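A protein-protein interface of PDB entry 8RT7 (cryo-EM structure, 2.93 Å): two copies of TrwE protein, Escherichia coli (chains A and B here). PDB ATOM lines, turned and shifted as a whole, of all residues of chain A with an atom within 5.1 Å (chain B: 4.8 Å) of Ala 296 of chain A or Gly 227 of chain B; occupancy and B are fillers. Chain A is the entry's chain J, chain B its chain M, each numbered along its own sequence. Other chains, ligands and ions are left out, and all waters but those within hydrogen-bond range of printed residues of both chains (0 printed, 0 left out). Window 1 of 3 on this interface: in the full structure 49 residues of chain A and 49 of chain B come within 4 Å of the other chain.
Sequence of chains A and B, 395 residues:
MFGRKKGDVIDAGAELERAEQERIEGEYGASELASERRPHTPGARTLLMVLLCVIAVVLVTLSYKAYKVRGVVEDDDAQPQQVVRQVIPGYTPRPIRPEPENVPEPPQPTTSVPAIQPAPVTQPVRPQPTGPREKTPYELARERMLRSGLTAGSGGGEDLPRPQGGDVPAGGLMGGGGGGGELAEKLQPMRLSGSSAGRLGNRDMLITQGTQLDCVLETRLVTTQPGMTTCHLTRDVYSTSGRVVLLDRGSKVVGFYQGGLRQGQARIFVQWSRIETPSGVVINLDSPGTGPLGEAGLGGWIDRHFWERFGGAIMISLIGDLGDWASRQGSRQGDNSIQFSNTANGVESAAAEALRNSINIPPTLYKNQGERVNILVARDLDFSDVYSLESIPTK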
ATOM      1  N   ARG A 267      25.818  -4.425 -27.331  1.00  0.00           N
ATOM      2  CA  ARG A 267      25.732  -4.995 -25.998  1.00  0.00           C
ATOM      3  C   ARG A 267      24.300  -5.433 -25.752  1.00  0.00           C
ATOM      4  O   ARG A 267      23.363  -4.758 -26.175  1.00  0.00           O
ATOM      5  CB  ARG A 267      26.151  -3.991 -24.928  1.00  0.00           C
ATOM      6  CG  ARG A 267      27.471  -3.313 -25.164  1.00  0.00           C
ATOM      7  CD  ARG A 267      27.859  -2.496 -23.987  1.00  0.00           C
ATOM      8  NE  ARG A 267      28.370  -3.337 -22.926  1.00  0.00           N
ATOM      9  CZ  ARG A 267      29.630  -3.711 -22.824  1.00  0.00           C
ATOM     10  NH1 ARG A 267      30.506  -3.312 -23.722  1.00  0.00           N
ATOM     11  NH2 ARG A 267      30.013  -4.481 -21.825  1.00  0.00           N
ATOM     12  N   PHE A 269      21.315  -6.684 -22.920  1.00  0.00           N
ATOM     13  CA  PHE A 269      20.944  -6.570 -21.518  1.00  0.00           C
ATOM     14  C   PHE A 269      20.769  -7.963 -20.948  1.00  0.00           C
ATOM     15  O   PHE A 269      19.915  -8.721 -21.410  1.00  0.00           O
ATOM     16  CB  PHE A 269      19.660  -5.769 -21.347  1.00  0.00           C
ATOM     17  CG  PHE A 269      19.399  -5.344 -19.937  1.00  0.00           C
ATOM     18  CD1 PHE A 269      18.723  -6.161 -19.064  1.00  0.00           C
ATOM     19  CD2 PHE A 269      19.828  -4.122 -19.488  1.00  0.00           C
ATOM     20  CE1 PHE A 269      18.496  -5.772 -17.780  1.00  0.00           C
ATOM     21  CE2 PHE A 269      19.595  -3.735 -18.201  1.00  0.00           C
ATOM     22  CZ  PHE A 269      18.933  -4.563 -17.348  1.00  0.00           C
ATOM     23  N   GLY A 289      23.478  -7.193 -15.452  1.00  0.00           N
ATOM     24  CA  GLY A 289      24.802  -7.706 -15.742  1.00  0.00           C
ATOM     25  C   GLY A 289      25.564  -6.685 -16.566  1.00  0.00           C
ATOM     26  O   GLY A 289      25.020  -6.097 -17.496  1.00  0.00           O
ATOM     27  N   THR A 290      26.823  -6.482 -16.209  1.00  0.00           N
ATOM     28  CA  THR A 290      27.628  -5.419 -16.775  1.00  0.00           C
ATOM     29  C   THR A 290      28.944  -6.004 -17.274  1.00  0.00           C
ATOM     30  O   THR A 290      29.209  -7.194 -17.130  1.00  0.00           O
ATOM     31  CB  THR A 290      27.860  -4.305 -15.743  1.00  0.00           C
ATOM     32  OG1 THR A 290      28.661  -4.799 -14.670  1.00  0.00           O
ATOM     33  CG2 THR A 290      26.552  -3.819 -15.168  1.00  0.00           C
ATOM     34  N   GLY A 291      29.768  -5.167 -17.882  1.00  0.00           N
ATOM     35  CA  GLY A 291      31.072  -5.583 -18.329  1.00  0.00           C
ATOM     36  C   GLY A 291      32.042  -5.629 -17.175  1.00  0.00           C
ATOM     37  O   GLY A 291      31.659  -5.452 -16.020  1.00  0.00           O
ATOM     38  N   GLY A 294      31.799  -2.256 -15.395  1.00  0.00           N
ATOM     39  CA  GLY A 294      30.519  -1.705 -15.043  1.00  0.00           C
ATOM     40  C   GLY A 294      29.710  -1.137 -16.176  1.00  0.00           C
ATOM     41  O   GLY A 294      28.657  -0.549 -15.917  1.00  0.00           O
ATOM     42  N   GLU A 295      30.153  -1.277 -17.416  1.00  0.00           N
ATOM     43  CA  GLU A 295      29.386  -0.745 -18.530  1.00  0.00           C
ATOM     44  C   GLU A 295      28.215  -1.666 -18.826  1.00  0.00           C
ATOM     45  O   GLU A 295      28.355  -2.888 -18.826  1.00  0.00           O
ATOM     46  CB  GLU A 295      30.268  -0.561 -19.760  1.00  0.00           C
ATOM     47  CG  GLU A 295      31.016  -1.774 -20.188  1.00  0.00           C
ATOM     48  CD  GLU A 295      32.443  -1.785 -19.727  1.00  0.00           C
ATOM     49  OE1 GLU A 295      32.673  -1.877 -18.515  1.00  0.00           O
ATOM     50  OE2 GLU A 295      33.346  -1.708 -20.575  1.00  0.00           O
ATOM     51  N   ALA A 296      27.053  -1.074 -19.070  1.00  0.00           N
ATOM     52  CA  ALA A 296      25.805  -1.816 -18.985  1.00  0.00           C
ATOM     53  C   ALA A 296      25.672  -2.817 -20.116  1.00  0.00           C
ATOM     54  O   ALA A 296      25.800  -2.465 -21.289  1.00  0.00           O
ATOM     55  CB  ALA A 296      24.624  -0.855 -19.004  1.00  0.00           C
ATOM     56  N   GLY A 297      25.384  -4.059 -19.761  1.00  0.00           N
ATOM     57  CA  GLY A 297      25.187  -5.114 -20.726  1.00  0.00           C
ATOM     58  C   GLY A 297      26.474  -5.847 -21.050  1.00  0.00           C
ATOM     59  O   GLY A 297      27.577  -5.337 -20.886  1.00  0.00           O
ATOM     60  N   LEU A 298      26.313  -7.078 -21.513  1.00  0.00           N
ATOM     61  CA  LEU A 298      27.435  -7.877 -21.979  1.00  0.00           C
ATOM     62  C   LEU A 298      27.694  -7.582 -23.445  1.00  0.00           C
ATOM     63  O   LEU A 298      26.759  -7.386 -24.219  1.00  0.00           O
ATOM     64  CB  LEU A 298      27.158  -9.365 -21.785  1.00  0.00           C
ATOM     65  CG  LEU A 298      27.419  -9.992 -20.421  1.00  0.00           C
ATOM     66  CD1 LEU A 298      26.467  -9.477 -19.399  1.00  0.00           C
ATOM     67  CD2 LEU A 298      27.259 -11.481 -20.530  1.00  0.00           C
ATOM     68  N   VAL B 222      28.598   3.120 -20.934  1.00  0.00           N
ATOM     69  CA  VAL B 222      28.240   2.993 -22.341  1.00  0.00           C
ATOM     70  C   VAL B 222      26.724   2.970 -22.410  1.00  0.00           C
ATOM     71  O   VAL B 222      26.090   2.179 -21.709  1.00  0.00           O
ATOM     72  CB  VAL B 222      28.830   1.725 -22.983  1.00  0.00           C
ATOM     73  CG1 VAL B 222      28.618   1.749 -24.468  1.00  0.00           C
ATOM     74  CG2 VAL B 222      30.288   1.594 -22.667  1.00  0.00           C
ATOM     75  N   GLN B 225      22.620   0.193 -23.565  1.00  0.00           N
ATOM     76  CA  GLN B 225      21.565  -0.428 -22.789  1.00  0.00           C
ATOM     77  C   GLN B 225      21.312   0.369 -21.522  1.00  0.00           C
ATOM     78  O   GLN B 225      22.238   0.971 -20.978  1.00  0.00           O
ATOM     79  CB  GLN B 225      21.937  -1.865 -22.410  1.00  0.00           C
ATOM     80  CG  GLN B 225      22.254  -2.760 -23.561  1.00  0.00           C
ATOM     81  CD  GLN B 225      21.030  -3.195 -24.317  1.00  0.00           C
ATOM     82  OE1 GLN B 225      19.916  -3.077 -23.834  1.00  0.00           O
ATOM     83  NE2 GLN B 225      21.234  -3.721 -25.510  1.00  0.00           N
ATOM     84  N   PRO B 226      20.080   0.389 -21.020  1.00  0.00           N
ATOM     85  CA  PRO B 226      19.831   1.032 -19.732  1.00  0.00           C
ATOM     86  C   PRO B 226      20.629   0.340 -18.649  1.00  0.00           C
ATOM     87  O   PRO B 226      20.908  -0.855 -18.723  1.00  0.00           O
ATOM     88  CB  PRO B 226      18.332   0.837 -19.527  1.00  0.00           C
ATOM     89  CG  PRO B 226      17.997  -0.305 -20.355  1.00  0.00           C
ATOM     90  CD  PRO B 226      18.854  -0.210 -21.555  1.00  0.00           C
ATOM     91  N   GLY B 227      21.019   1.098 -17.641  1.00  0.00           N
ATOM     92  CA  GLY B 227      21.910   0.488 -16.680  1.00  0.00           C
ATOM     93  C   GLY B 227      21.996   1.322 -15.434  1.00  0.00           C
ATOM     94  O   GLY B 227      21.339   2.352 -15.301  1.00  0.00           O
ATOM     95  N   MET B 228      22.817   0.848 -14.514  1.00  0.00           N
ATOM     96  CA  MET B 228      22.996   1.489 -13.230  1.00  0.00           C
ATOM     97  C   MET B 228      24.440   1.926 -13.095  1.00  0.00           C
ATOM     98  O   MET B 228      25.353   1.209 -13.502  1.00  0.00           O
ATOM     99  CB  MET B 228      22.604   0.557 -12.100  1.00  0.00           C
ATOM    100  CG  MET B 228      21.134   0.248 -12.090  1.00  0.00           C
ATOM    101  SD  MET B 228      20.685  -0.902 -10.813  1.00  0.00           S
ATOM    102  CE  MET B 228      20.913   0.139  -9.391  1.00  0.00           C
ATOM    103  N   THR B 229      24.637   3.115 -12.549  1.00  0.00           N
ATOM    104  CA  THR B 229      25.948   3.713 -12.378  1.00  0.00           C
ATOM    105  C   THR B 229      26.321   3.703 -10.904  1.00  0.00           C
ATOM    106  O   THR B 229      25.538   3.311 -10.044  1.00  0.00           O
ATOM    107  CB  THR B 229      25.970   5.140 -12.931  1.00  0.00           C
ATOM    108  OG1 THR B 229      25.072   5.954 -12.182  1.00  0.00           O
ATOM    109  CG2 THR B 229      25.514   5.159 -14.355  1.00  0.00           C
ATOM    110  N   GLY B 255      22.992   5.215  -9.004  1.00  0.00           N
ATOM    111  CA  GLY B 255      22.085   5.900  -9.896  1.00  0.00           C
ATOM    112  C   GLY B 255      21.846   5.082 -11.140  1.00  0.00           C
ATOM    113  O   GLY B 255      22.326   3.961 -11.262  1.00  0.00           O
ATOM    114  N   PHE B 256      21.084   5.645 -12.069  1.00  0.00           N
ATOM    115  CA  PHE B 256      20.777   4.925 -13.291  1.00  0.00           C
ATOM    116  C   PHE B 256      20.453   5.904 -14.402  1.00  0.00           C
ATOM    117  O   PHE B 256      20.019   7.027 -14.159  1.00  0.00           O
ATOM    118  CB  PHE B 256      19.610   3.962 -13.093  1.00  0.00           C
ATOM    119  CG  PHE B 256      18.298   4.638 -12.881  1.00  0.00           C
ATOM    120  CD1 PHE B 256      17.947   5.102 -11.643  1.00  0.00           C
ATOM    121  CD2 PHE B 256      17.409   4.793 -13.918  1.00  0.00           C
ATOM    122  CE1 PHE B 256      16.756   5.711 -11.449  1.00  0.00           C
ATOM    123  CE2 PHE B 256      16.214   5.412 -13.718  1.00  0.00           C
ATOM    124  CZ  PHE B 256      15.889   5.866 -12.485  1.00  0.00           C
ATOM    125  N   TYR B 257      20.653   5.445 -15.627  1.00  0.00           N
ATOM    126  CA  TYR B 257      20.244   6.158 -16.823  1.00  0.00           C
ATOM    127  C   TYR B 257      19.367   5.243 -17.660  1.00  0.00           C
ATOM    128  O   TYR B 257      19.317   4.034 -17.449  1.00  0.00           O
ATOM    129  CB  TYR B 257      21.452   6.621 -17.631  1.00  0.00           C
ATOM    130  CG  TYR B 257      22.318   5.489 -18.096  1.00  0.00           C
ATOM    131  CD1 TYR B 257      23.334   5.003 -17.300  1.00  0.00           C
ATOM    132  CD2 TYR B 257      22.118   4.901 -19.330  1.00  0.00           C
ATOM    133  CE1 TYR B 257      24.115   3.971 -17.717  1.00  0.00           C
ATOM    134  CE2 TYR B 257      22.892   3.870 -19.746  1.00  0.00           C
ATOM    135  CZ  TYR B 257      23.889   3.408 -18.938  1.00  0.00           C
ATOM    136  OH  TYR B 257      24.675   2.373 -19.363  1.00  0.00           O
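O of Arg 267 of chain A lies within hydrogen-bond range of NE2 of Gln 225 of chain B.
NH2 of Arg 267 of chain A lies within hydrogen-bond range of O of Gly 297 of chain A (2.7 Å).
O of Val 222 of chain B is in hydrogen-bond range of OH of Tyr 257 of chain B (2.7 Å).
The guanidinium group (NE) of Arg 267 of chain A lies within hydrogen-bond range of the backbone carbonyl oxygen (O) of Ala 296 of chain A (3.2 Å).
The side-chain hydroxyl (OH) of Tyr 257 of chain B sits close to the backbone carbonyl oxygen (O) of Gln 225 of chain B.
O of Gly 227 of chain B is in hydrogen-bond range of N of Tyr 257 of chain B (3.2 Å).
Among the printed residues, pairs that only touch across the chains: Phe 269 of chain A with Pro 226 of chain B, Ala 296 of chain A with Tyr 257 of chain B, Ala 296 of chain A with Gln 225 of chain B, Glu 295 of chain A with Val 222 of chain B, Phe 269 of chain A with Gln 225 of chain B, Ala 296 of chain A with Pro 226 of chain B and Ala 296 of chain A with Gly 227 of chain B.
Gly 289 of chain A touches none of the printed residues of chain B.
Of chain B, only Gln 225, Pro 226, Gly 227 and Tyr 257 come within 4 Å of Ala 296 of chain A.
Of the printed residues of chain A, Val 222 of chain B touches Glu 295.
Printed residues of chain A within 4 Å of Gln 225 of chain B: Arg 267, Phe 269 and Ala 296.
Gly 227 of chain B touches just one residue of chain A: Ala 296 (3.8 Å).
Of the printed residues of chain A, Tyr 257 of chain B touches Ala 296.
The nearest residue of chain B that does not touch Ala 296 of chain A is Val 222 of chain B (4.3 Å).
The nearest printed residue of chain B that does not touch Arg 267 of chain A is Val 222 of chain B (4.3 Å).
Of the 9 printed residues of chain B, 5 touch a printed residue of chain A.
Hydrophobic or aromatic side chains of chain B within 4 Å of the printed part of chain A: Val 222 and Tyr 257.
Along chain B the printed residues that touch a printed residue of chain A span positions 222 to 257.
Printed residues of chain A that touch a printed residue of chain B: Arg 267, Phe 269, Glu 295 and Ala 296.
Hydrophobic or aromatic side chains of chain A within 4 Å of the printed part of chain B: Phe 269 and Ala 296.
Among the printed residues, 8 pairs touch across the chains.
Among the printed residues, no Asp or Glu carboxylate lies within 4 Å of a Lys or Arg side-chain nitrogen of the other chain.
No position is printed for both chains.
Of the 8 pairs that touch across the chains among the printed residues, none has its exchanged pair printed and touching as well.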
